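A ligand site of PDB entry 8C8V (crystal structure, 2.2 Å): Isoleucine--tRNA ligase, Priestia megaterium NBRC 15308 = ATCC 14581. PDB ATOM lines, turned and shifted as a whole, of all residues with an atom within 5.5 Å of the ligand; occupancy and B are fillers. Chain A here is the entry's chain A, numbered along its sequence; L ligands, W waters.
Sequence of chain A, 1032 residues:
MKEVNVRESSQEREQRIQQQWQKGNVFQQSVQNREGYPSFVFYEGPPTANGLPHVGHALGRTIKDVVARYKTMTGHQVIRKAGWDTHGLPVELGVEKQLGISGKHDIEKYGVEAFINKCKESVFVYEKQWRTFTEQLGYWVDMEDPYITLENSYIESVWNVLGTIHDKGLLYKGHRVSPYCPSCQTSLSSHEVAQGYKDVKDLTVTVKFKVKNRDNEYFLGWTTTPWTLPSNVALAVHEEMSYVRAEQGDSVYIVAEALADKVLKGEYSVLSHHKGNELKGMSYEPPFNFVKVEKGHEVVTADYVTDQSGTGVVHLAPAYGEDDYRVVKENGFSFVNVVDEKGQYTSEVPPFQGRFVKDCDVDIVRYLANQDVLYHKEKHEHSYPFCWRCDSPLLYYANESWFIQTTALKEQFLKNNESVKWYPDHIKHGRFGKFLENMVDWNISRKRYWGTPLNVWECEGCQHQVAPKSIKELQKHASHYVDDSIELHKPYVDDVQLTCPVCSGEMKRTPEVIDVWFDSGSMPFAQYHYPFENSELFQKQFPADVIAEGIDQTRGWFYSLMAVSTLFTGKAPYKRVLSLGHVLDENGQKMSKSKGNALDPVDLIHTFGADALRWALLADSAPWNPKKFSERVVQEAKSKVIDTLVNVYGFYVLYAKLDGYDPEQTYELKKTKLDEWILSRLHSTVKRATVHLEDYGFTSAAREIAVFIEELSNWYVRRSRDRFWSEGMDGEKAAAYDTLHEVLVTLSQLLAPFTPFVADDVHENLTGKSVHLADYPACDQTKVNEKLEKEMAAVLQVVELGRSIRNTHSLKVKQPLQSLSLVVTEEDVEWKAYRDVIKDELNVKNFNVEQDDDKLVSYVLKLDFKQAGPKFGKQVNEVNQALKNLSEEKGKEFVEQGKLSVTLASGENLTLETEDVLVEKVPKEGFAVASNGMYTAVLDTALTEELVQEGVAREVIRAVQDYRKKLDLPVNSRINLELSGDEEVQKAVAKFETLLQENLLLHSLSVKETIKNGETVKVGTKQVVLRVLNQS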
ATOM      1  N   GLY A  45      28.411   8.565 -13.589  1.00  0.00           N
ATOM      2  CA  GLY A  45      28.304   7.380 -14.404  1.00  0.00           C
ATOM      3  C   GLY A  45      26.912   7.282 -14.999  1.00  0.00           C
ATOM      4  O   GLY A  45      25.920   7.319 -14.265  1.00  0.00           O
ATOM      5  N   PRO A  46      26.815   7.137 -16.315  1.00  0.00           N
ATOM      6  CA  PRO A  46      25.515   7.301 -16.992  1.00  0.00           C
ATOM      7  C   PRO A  46      24.685   6.036 -16.913  1.00  0.00           C
ATOM      8  O   PRO A  46      25.069   4.995 -17.443  1.00  0.00           O
ATOM      9  CB  PRO A  46      25.919   7.604 -18.446  1.00  0.00           C
ATOM     10  CG  PRO A  46      27.221   6.836 -18.625  1.00  0.00           C
ATOM     11  CD  PRO A  46      27.913   6.839 -17.254  1.00  0.00           C
ATOM     12  N   PRO A  47      23.516   6.095 -16.265  1.00  0.00           N
ATOM     13  CA  PRO A  47      22.637   4.918 -16.219  1.00  0.00           C
ATOM     14  C   PRO A  47      22.187   4.497 -17.607  1.00  0.00           C
ATOM     15  O   PRO A  47      21.911   5.333 -18.466  1.00  0.00           O
ATOM     16  CB  PRO A  47      21.457   5.386 -15.369  1.00  0.00           C
ATOM     17  CG  PRO A  47      21.996   6.529 -14.558  1.00  0.00           C
ATOM     18  CD  PRO A  47      22.984   7.218 -15.473  1.00  0.00           C
ATOM     19  N   THR A  48      22.093   3.186 -17.813  1.00  0.00           N
ATOM     20  CA  THR A  48      21.587   2.660 -19.068  1.00  0.00           C
ATOM     21  C   THR A  48      20.091   2.863 -19.152  1.00  0.00           C
ATOM     22  O   THR A  48      19.346   2.447 -18.254  1.00  0.00           O
ATOM     23  CB  THR A  48      21.916   1.170 -19.184  1.00  0.00           C
ATOM     24  OG1 THR A  48      23.325   0.977 -19.101  1.00  0.00           O
ATOM     25  CG2 THR A  48      21.403   0.625 -20.516  1.00  0.00           C
ATOM     26  N   HIS A  54      15.279   0.789  -9.898  1.00  0.00           N
ATOM     27  CA  HIS A  54      14.860   0.099  -8.685  1.00  0.00           C
ATOM     28  C   HIS A  54      15.636   0.661  -7.501  1.00  0.00           C
ATOM     29  O   HIS A  54      16.497   1.535  -7.654  1.00  0.00           O
ATOM     30  CB  HIS A  54      15.019  -1.425  -8.828  1.00  0.00           C
ATOM     31  CG  HIS A  54      16.417  -1.873  -9.140  1.00  0.00           C
ATOM     32  ND1 HIS A  54      17.499  -1.562  -8.347  1.00  0.00           N
ATOM     33  CD2 HIS A  54      16.893  -2.627 -10.151  1.00  0.00           C
ATOM     34  CE1 HIS A  54      18.585  -2.103  -8.861  1.00  0.00           C
ATOM     35  NE2 HIS A  54      18.252  -2.749  -9.963  1.00  0.00           N
ATOM     36  N   GLY A  56      17.916  -0.420  -5.666  1.00  0.00           N
ATOM     37  CA  GLY A  56      19.363  -0.553  -5.705  1.00  0.00           C
ATOM     38  C   GLY A  56      20.039   0.632  -6.369  1.00  0.00           C
ATOM     39  O   GLY A  56      21.119   1.051  -5.965  1.00  0.00           O
ATOM     40  N   HIS A  57      19.392   1.198  -7.399  1.00  0.00           N
ATOM     41  CA  HIS A  57      19.922   2.390  -8.050  1.00  0.00           C
ATOM     42  C   HIS A  57      19.848   3.620  -7.166  1.00  0.00           C
ATOM     43  O   HIS A  57      20.586   4.580  -7.395  1.00  0.00           O
ATOM     44  CB  HIS A  57      19.167   2.656  -9.362  1.00  0.00           C
ATOM     45  CG  HIS A  57      19.229   1.518 -10.330  1.00  0.00           C
ATOM     46  ND1 HIS A  57      18.105   0.961 -10.889  1.00  0.00           N
ATOM     47  CD2 HIS A  57      20.284   0.836 -10.836  1.00  0.00           C
ATOM     48  CE1 HIS A  57      18.469  -0.019 -11.714  1.00  0.00           C
ATOM     49  NE2 HIS A  57      19.784  -0.106 -11.697  1.00  0.00           N
ATOM     50  N   LEU A  59      20.818   3.722  -4.089  1.00  0.00           N
ATOM     51  CA  LEU A  59      21.989   3.773  -3.216  1.00  0.00           C
ATOM     52  C   LEU A  59      23.091   4.631  -3.819  1.00  0.00           C
ATOM     53  O   LEU A  59      23.587   5.563  -3.174  1.00  0.00           O
ATOM     54  CB  LEU A  59      22.508   2.354  -2.931  1.00  0.00           C
ATOM     55  CG  LEU A  59      23.813   2.264  -2.141  1.00  0.00           C
ATOM     56  CD1 LEU A  59      23.686   2.898  -0.760  1.00  0.00           C
ATOM     57  CD2 LEU A  59      24.307   0.815  -2.012  1.00  0.00           C
ATOM     58  N   ASP A  85      23.234   6.531 -20.775  1.00  0.00           N
ATOM     59  CA  ASP A  85      23.908   5.531 -21.609  1.00  0.00           C
ATOM     60  C   ASP A  85      22.859   4.878 -22.505  1.00  0.00           C
ATOM     61  O   ASP A  85      21.940   4.230 -21.998  1.00  0.00           O
ATOM     62  CB  ASP A  85      24.570   4.504 -20.690  1.00  0.00           C
ATOM     63  CG  ASP A  85      25.769   3.824 -21.325  1.00  0.00           C
ATOM     64  OD1 ASP A  85      26.019   4.031 -22.530  1.00  0.00           O
ATOM     65  OD2 ASP A  85      26.457   3.075 -20.600  1.00  0.00           O
ATOM     66  N   TRP A 130      13.865   7.839 -15.428  1.00  0.00           N
ATOM     67  CA  TRP A 130      15.039   8.002 -14.572  1.00  0.00           C
ATOM     68  C   TRP A 130      15.148   9.438 -14.055  1.00  0.00           C
ATOM     69  O   TRP A 130      15.534   9.658 -12.902  1.00  0.00           O
ATOM     70  CB  TRP A 130      16.296   7.593 -15.324  1.00  0.00           C
ATOM     71  CG  TRP A 130      16.599   6.139 -15.200  1.00  0.00           C
ATOM     72  CD1 TRP A 130      16.051   5.116 -15.912  1.00  0.00           C
ATOM     73  CD2 TRP A 130      17.529   5.537 -14.285  1.00  0.00           C
ATOM     74  NE1 TRP A 130      16.575   3.916 -15.516  1.00  0.00           N
ATOM     75  CE2 TRP A 130      17.489   4.144 -14.513  1.00  0.00           C
ATOM     76  CE3 TRP A 130      18.392   6.031 -13.300  1.00  0.00           C
ATOM     77  CZ2 TRP A 130      18.273   3.242 -13.788  1.00  0.00           C
ATOM     78  CZ3 TRP A 130      19.169   5.147 -12.586  1.00  0.00           C
ATOM     79  CH2 TRP A 130      19.108   3.766 -12.842  1.00  0.00           C
ATOM     80  N   TRP A 517      30.651  -0.158 -23.656  1.00  0.00           N
ATOM     81  CA  TRP A 517      31.497   0.300 -22.568  1.00  0.00           C
ATOM     82  C   TRP A 517      32.490   1.363 -23.020  1.00  0.00           C
ATOM     83  O   TRP A 517      32.934   2.174 -22.199  1.00  0.00           O
ATOM     84  CB  TRP A 517      32.237  -0.891 -21.955  1.00  0.00           C
ATOM     85  CG  TRP A 517      31.340  -1.788 -21.177  1.00  0.00           C
ATOM     86  CD1 TRP A 517      30.962  -3.054 -21.499  1.00  0.00           C
ATOM     87  CD2 TRP A 517      30.689  -1.469 -19.944  1.00  0.00           C
ATOM     88  NE1 TRP A 517      30.122  -3.549 -20.545  1.00  0.00           N
ATOM     89  CE2 TRP A 517      29.934  -2.606 -19.570  1.00  0.00           C
ATOM     90  CE3 TRP A 517      30.676  -0.342 -19.112  1.00  0.00           C
ATOM     91  CZ2 TRP A 517      29.180  -2.637 -18.405  1.00  0.00           C
ATOM     92  CZ3 TRP A 517      29.910  -0.388 -17.963  1.00  0.00           C
ATOM     93  CH2 TRP A 517      29.169  -1.524 -17.613  1.00  0.00           C
ATOM     94  N   SER A 520      30.714   4.950 -22.608  1.00  0.00           N
ATOM     95  CA  SER A 520      30.718   5.520 -21.260  1.00  0.00           C
ATOM     96  C   SER A 520      32.129   5.789 -20.768  1.00  0.00           C
ATOM     97  O   SER A 520      32.385   6.789 -20.097  1.00  0.00           O
ATOM     98  CB  SER A 520      29.973   4.594 -20.296  1.00  0.00           C
ATOM     99  OG  SER A 520      30.586   3.312 -20.221  1.00  0.00           O
ATOM    100  N   ALA A 548      31.554   7.201  -7.979  1.00  0.00           N
ATOM    101  CA  ALA A 548      30.892   6.281  -7.057  1.00  0.00           C
ATOM    102  C   ALA A 548      29.824   5.502  -7.815  1.00  0.00           C
ATOM    103  O   ALA A 548      28.780   6.055  -8.176  1.00  0.00           O
ATOM    104  CB  ALA A 548      30.296   7.034  -5.861  1.00  0.00           C
ATOM    105  N   GLU A 549      30.093   4.222  -8.062  1.00  0.00           N
ATOM    106  CA  GLU A 549      29.182   3.349  -8.782  1.00  0.00           C
ATOM    107  C   GLU A 549      29.314   1.948  -8.198  1.00  0.00           C
ATOM    108  O   GLU A 549      30.173   1.684  -7.358  1.00  0.00           O
ATOM    109  CB  GLU A 549      29.468   3.340 -10.295  1.00  0.00           C
ATOM    110  CG  GLU A 549      29.521   4.716 -10.961  1.00  0.00           C
ATOM    111  CD  GLU A 549      28.168   5.408 -11.029  1.00  0.00           C
ATOM    112  OE1 GLU A 549      27.133   4.711 -11.100  1.00  0.00           O
ATOM    113  OE2 GLU A 549      28.135   6.661 -11.022  1.00  0.00           O
ATOM    114  N   GLY A 550      28.449   1.038  -8.663  1.00  0.00           N
ATOM    115  CA  GLY A 550      28.400  -0.296  -8.108  1.00  0.00           C
ATOM    116  C   GLY A 550      29.628  -1.127  -8.447  1.00  0.00           C
ATOM    117  O   GLY A 550      30.359  -0.865  -9.401  1.00  0.00           O
ATOM    118  N   ILE A 551      29.831  -2.182  -7.641  1.00  0.00           N
ATOM    119  CA  ILE A 551      31.026  -3.011  -7.754  1.00  0.00           C
ATOM    120  C   ILE A 551      31.129  -3.670  -9.126  1.00  0.00           C
ATOM    121  O   ILE A 551      32.240  -3.993  -9.575  1.00  0.00           O
ATOM    122  CB  ILE A 551      31.053  -4.067  -6.625  1.00  0.00           C
ATOM    123  CG1 ILE A 551      32.405  -4.781  -6.575  1.00  0.00           C
ATOM    124  CG2 ILE A 551      29.911  -5.078  -6.789  1.00  0.00           C
ATOM    125  CD1 ILE A 551      32.562  -5.773  -5.424  1.00  0.00           C
ATOM    126  N   ASP A 552      30.004  -3.859  -9.823  1.00  0.00           N
ATOM    127  CA  ASP A 552      30.073  -4.480 -11.140  1.00  0.00           C
ATOM    128  C   ASP A 552      30.841  -3.614 -12.142  1.00  0.00           C
ATOM    129  O   ASP A 552      31.309  -4.143 -13.164  1.00  0.00           O
ATOM    130  CB  ASP A 552      28.666  -4.772 -11.670  1.00  0.00           C
ATOM    131  CG  ASP A 552      27.757  -3.552 -11.644  1.00  0.00           C
ATOM    132  OD1 ASP A 552      27.599  -2.952 -10.552  1.00  0.00           O
ATOM    133  OD2 ASP A 552      27.201  -3.194 -12.696  1.00  0.00           O
ATOM    134  N   GLN A 553      31.012  -2.330 -11.866  1.00  0.00           N
ATOM    135  CA  GLN A 553      31.792  -1.494 -12.773  1.00  0.00           C
ATOM    136  C   GLN A 553      33.285  -1.805 -12.745  1.00  0.00           C
ATOM    137  O   GLN A 553      34.009  -1.310 -13.618  1.00  0.00           O
ATOM    138  CB  GLN A 553      31.573  -0.010 -12.454  1.00  0.00           C
ATOM    139  CG  GLN A 553      30.101   0.415 -12.432  1.00  0.00           C
ATOM    140  CD  GLN A 553      29.343   0.025 -13.687  1.00  0.00           C
ATOM    141  OE1 GLN A 553      29.896  -0.017 -14.792  1.00  0.00           O
ATOM    142  NE2 GLN A 553      28.047  -0.250 -13.530  1.00  0.00           N
ATOM    143  N   TRP A 557      32.431   0.329 -16.050  1.00  0.00           N
ATOM    144  CA  TRP A 557      32.797   1.730 -16.245  1.00  0.00           C
ATOM    145  C   TRP A 557      34.154   2.041 -15.612  1.00  0.00           C
ATOM    146  O   TRP A 557      34.944   2.806 -16.188  1.00  0.00           O
ATOM    147  CB  TRP A 557      31.715   2.629 -15.671  1.00  0.00           C
ATOM    148  CG  TRP A 557      31.792   4.076 -16.073  1.00  0.00           C
ATOM    149  CD1 TRP A 557      31.891   4.572 -17.336  1.00  0.00           C
ATOM    150  CD2 TRP A 557      31.758   5.212 -15.196  1.00  0.00           C
ATOM    151  NE1 TRP A 557      31.931   5.946 -17.313  1.00  0.00           N
ATOM    152  CE2 TRP A 557      31.850   6.367 -16.005  1.00  0.00           C
ATOM    153  CE3 TRP A 557      31.660   5.368 -13.812  1.00  0.00           C
ATOM    154  CZ2 TRP A 557      31.849   7.655 -15.470  1.00  0.00           C
ATOM    155  CZ3 TRP A 557      31.658   6.644 -13.286  1.00  0.00           C
ATOM    156  CH2 TRP A 557      31.750   7.777 -14.112  1.00  0.00           C
ATOM    157  N   GLY A 581      28.639  -1.913  -2.860  1.00  0.00           N
ATOM    158  CA  GLY A 581      27.981  -3.206  -2.870  1.00  0.00           C
ATOM    159  C   GLY A 581      26.545  -3.098  -3.350  1.00  0.00           C
ATOM    160  O   GLY A 581      25.886  -2.074  -3.178  1.00  0.00           O
ATOM    161  N   HIS A 582      26.062  -4.170  -3.977  1.00  0.00           N
ATOM    162  CA  HIS A 582      24.723  -4.181  -4.545  1.00  0.00           C
ATOM    163  C   HIS A 582      23.658  -4.346  -3.462  1.00  0.00           C
ATOM    164  O   HIS A 582      23.850  -5.089  -2.492  1.00  0.00           O
ATOM    165  CB  HIS A 582      24.574  -5.303  -5.578  1.00  0.00           C
ATOM    166  CG  HIS A 582      25.104  -4.949  -6.924  1.00  0.00           C
ATOM    167  ND1 HIS A 582      24.881  -5.735  -8.041  1.00  0.00           N
ATOM    168  CD2 HIS A 582      25.840  -3.894  -7.354  1.00  0.00           C
ATOM    169  CE1 HIS A 582      25.459  -5.177  -9.087  1.00  0.00           C
ATOM    170  NE2 HIS A 582      26.056  -4.059  -8.702  1.00  0.00           N
ATOM    171  N   VAL A 583      22.539  -3.661  -3.648  1.00  0.00           N
ATOM    172  CA  VAL A 583      21.374  -3.839  -2.788  1.00  0.00           C
ATOM    173  C   VAL A 583      20.668  -5.138  -3.170  1.00  0.00           C
ATOM    174  O   VAL A 583      20.405  -5.383  -4.359  1.00  0.00           O
ATOM    175  CB  VAL A 583      20.417  -2.634  -2.903  1.00  0.00           C
ATOM    176  CG1 VAL A 583      19.112  -2.931  -2.179  1.00  0.00           C
ATOM    177  CG2 VAL A 583      21.061  -1.395  -2.330  1.00  0.00           C
ATOM    178  N   LYS A 590      19.316 -11.355  -5.072  1.00  0.00           N
ATOM    179  CA  LYS A 590      19.569 -10.243  -5.986  1.00  0.00           C
ATOM    180  C   LYS A 590      18.265  -9.686  -6.523  1.00  0.00           C
ATOM    181  O   LYS A 590      17.294 -10.423  -6.739  1.00  0.00           O
ATOM    182  CB  LYS A 590      20.474 -10.701  -7.134  1.00  0.00           C
ATOM    183  CG  LYS A 590      20.913  -9.576  -8.054  1.00  0.00           C
ATOM    184  CD  LYS A 590      21.671  -8.507  -7.275  1.00  0.00           C
ATOM    185  CE  LYS A 590      22.009  -7.322  -8.169  1.00  0.00           C
ATOM    186  NZ  LYS A 590      22.728  -7.729  -9.415  1.00  0.00           N
ATOM    187  N   MET A 591      18.233  -8.371  -6.733  1.00  0.00           N
ATOM    188  CA  MET A 591      17.012  -7.689  -7.143  1.00  0.00           C
ATOM    189  C   MET A 591      16.821  -7.780  -8.643  1.00  0.00           C
ATOM    190  O   MET A 591      17.735  -7.510  -9.425  1.00  0.00           O
ATOM    191  CB  MET A 591      17.060  -6.223  -6.709  1.00  0.00           C
ATOM    192  CG  MET A 591      16.839  -6.016  -5.231  1.00  0.00           C
ATOM    193  SD  MET A 591      16.863  -4.269  -4.823  1.00  0.00           S
ATOM    194  CE  MET A 591      15.925  -3.630  -6.200  1.00  0.00           C
HETATM  195  N1  LIG L   1      25.384   2.433 -17.946  1.00  0.00           N
HETATM  196  C1  LIG L   1      26.236   1.517 -17.214  1.00  0.00           C
HETATM  197  C2  LIG L   1      27.443   2.188 -16.536  1.00  0.00           C
HETATM  198  C3  LIG L   1      28.199   3.061 -17.536  1.00  0.00           C
HETATM  199  C4  LIG L   1      26.987   2.995 -15.330  1.00  0.00           C
HETATM  200  C5  LIG L   1      28.119   3.570 -14.495  1.00  0.00           C
HETATM  201  C6  LIG L   1      25.350   0.865 -16.164  1.00  0.00           C
HETATM  202  O1  LIG L   1      25.705  -0.094 -15.503  1.00  0.00           O
HETATM  203  S1  LIG L   1      22.972   0.825 -14.906  1.00  0.00           S
HETATM  204  O2  LIG L   1      21.868   1.749 -15.006  1.00  0.00           O
HETATM  205  O3  LIG L   1      22.788  -0.585 -15.170  1.00  0.00           O
HETATM  206  N2  LIG L   1      24.112   1.409 -16.008  1.00  0.00           N
HETATM  207  N3  LIG L   1      23.596   0.957 -13.413  1.00  0.00           N
HETATM  208  C7  LIG L   1      23.415   2.199 -12.682  1.00  0.00           C
HETATM  209  C8  LIG L   1      24.230   2.151 -11.406  1.00  0.00           C
HETATM  210  O4  LIG L   1      23.597   1.292 -10.448  1.00  0.00           O
HETATM  211  C9  LIG L   1      24.458   0.267 -10.035  1.00  0.00           C
HETATM  212  N4  LIG L   1      23.656  -0.888  -9.730  1.00  0.00           N
HETATM  213  C10 LIG L   1      23.306  -1.300  -8.471  1.00  0.00           C
HETATM  214  N5  LIG L   1      23.632  -0.743  -7.313  1.00  0.00           N
HETATM  215  C11 LIG L   1      23.126  -1.409  -6.280  1.00  0.00           C
HETATM  216  N6  LIG L   1      22.367  -2.501  -6.306  1.00  0.00           N
HETATM  217  C12 LIG L   1      22.032  -3.041  -7.486  1.00  0.00           C
HETATM  218  N7  LIG L   1      21.269  -4.133  -7.491  1.00  0.00           N
HETATM  219  C13 LIG L   1      22.510  -2.426  -8.661  1.00  0.00           C
HETATM  220  N8  LIG L   1      22.363  -2.708  -9.997  1.00  0.00           N
HETATM  221  C14 LIG L   1      23.057  -1.772 -10.596  1.00  0.00           C
HETATM  222  C15 LIG L   1      25.478   0.127 -11.176  1.00  0.00           C
HETATM  223  O5  LIG L   1      26.669  -0.448 -10.754  1.00  0.00           O
HETATM  224  C16 LIG L   1      25.641   1.592 -11.602  1.00  0.00           C
HETATM  225  O6  LIG L   1      26.491   2.240 -10.699  1.00  0.00           O
HETATM  226  O   HOH W   1      23.584   2.435  -6.978  1.00  0.00           O
HETATM  227  O   HOH W   2      22.729   4.276  -9.085  1.00  0.00           O
HETATM  228  O   HOH W   3      25.126   5.137 -12.799  1.00  0.00           O
HETATM  229  O   HOH W   4      22.066  -5.784 -11.241  1.00  0.00           O
HETATM  230  O   HOH W   5      24.662  -2.225 -13.631  1.00  0.00           O
HETATM  231  O   HOH W   6      19.394   0.546 -15.818  1.00  0.00           O
HETATM  232  O   HOH W   7      27.106  -0.379 -19.999  1.00  0.00           O
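An oxygen (O6) of the ligand sits at hydrogen-bond distance from the side-chain carboxylate (OE1) of Glu 549, 2.6 Å away.
O of Pro 46 is in hydrogen-bond range of N1 of the ligand (2.6 Å).
OD1 of Asp 552 lies within hydrogen-bond range of O5 of the ligand.
The backbone NH of Thr 48 is in hydrogen-bond range of an oxygen (O2) of the ligand, at 3.2 Å.
N1 of the ligand sits at hydrogen-bond distance from OG1 of Thr 48 (2.8 Å).
N6 of the ligand lies within hydrogen-bond range of N of Val 583 (2.9 Å).
The backbone carbonyl oxygen (O) of Val 583 sits at hydrogen-bond distance from a nitrogen (N7) of the ligand, 3.5 Å away.
The side-chain carboxylate (OD2) of Asp 85 lies within salt-bridge range of a nitrogen (N1) of the ligand (2.9 Å).
O1 of the ligand is in hydrogen-bond range of NE2 of Gln 553.
An oxygen (O6) of the ligand is in hydrogen-bond range of the backbone NH (N) of Gly 550 (3.1 Å).
N of Gly 45 sits at hydrogen-bond distance from OE2 of Glu 549 (3.2 Å).
The side-chain carboxylate (OD1) of Asp 552 sits at hydrogen-bond distance from a ring nitrogen (NE2) of His 582 (2.7 Å).
N of Asp 85 lies within hydrogen-bond range of O of Pro 47 (2.9 Å).
The side-chain amide oxygen (OE1) of Gln 553 sits at hydrogen-bond distance from the backbone NH (N) of Trp 557 (2.9 Å).
The backbone NH (N) of Gly 56 sits at hydrogen-bond distance from a ring nitrogen (ND1) of His 54, at 2.9 Å.
ND1 of His 582 is in hydrogen-bond range of NZ of Lys 590.
A ring nitrogen (ND1) of His 57 sits at hydrogen-bond distance from the backbone NH (N) of His 54.
The side-chain hydroxyl of Ser 520 lies within hydrogen-bond range of the backbone carbonyl oxygen of Trp 517 (3.3 Å).
The backbone carbonyl oxygen of Gly 56 sits close to a nitrogen (N5) of the ligand, 3.4 Å away.
Residues that only touch the ligand: Gly 45, Pro 47, His 54, His 57, Trp 517, Ser 520, Trp 557, His 582 and Lys 590.
Of the 24 residues printed, 18 come within 4 Å of the ligand.
The nearest printed residue that does not touch the ligand is Trp 130 (4.05 Å).
Water W6 lies within hydrogen-bond range of O2 of the ligand (2.9 Å) and O of Thr 48 (3.1 Å).
Water W5 bridges the side-chain carboxylate (OD2) of Asp 552 and an oxygen (O3) of the ligand.
Water W1 lies within hydrogen-bond range of the backbone carbonyl oxygen (O) of Gly 56 (3.0 Å) and a nitrogen (N5) of the ligand (3.2 Å).
Water W4 lies within hydrogen-bond range of NZ of Lys 590 (2.7 Å) and N8 of the ligand (3.3 Å).
Water W2 lies within hydrogen-bond range of O of His 57 and O4 of the ligand.
Water W3 bridges OE1 of Glu 549 and O of Gly 45.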
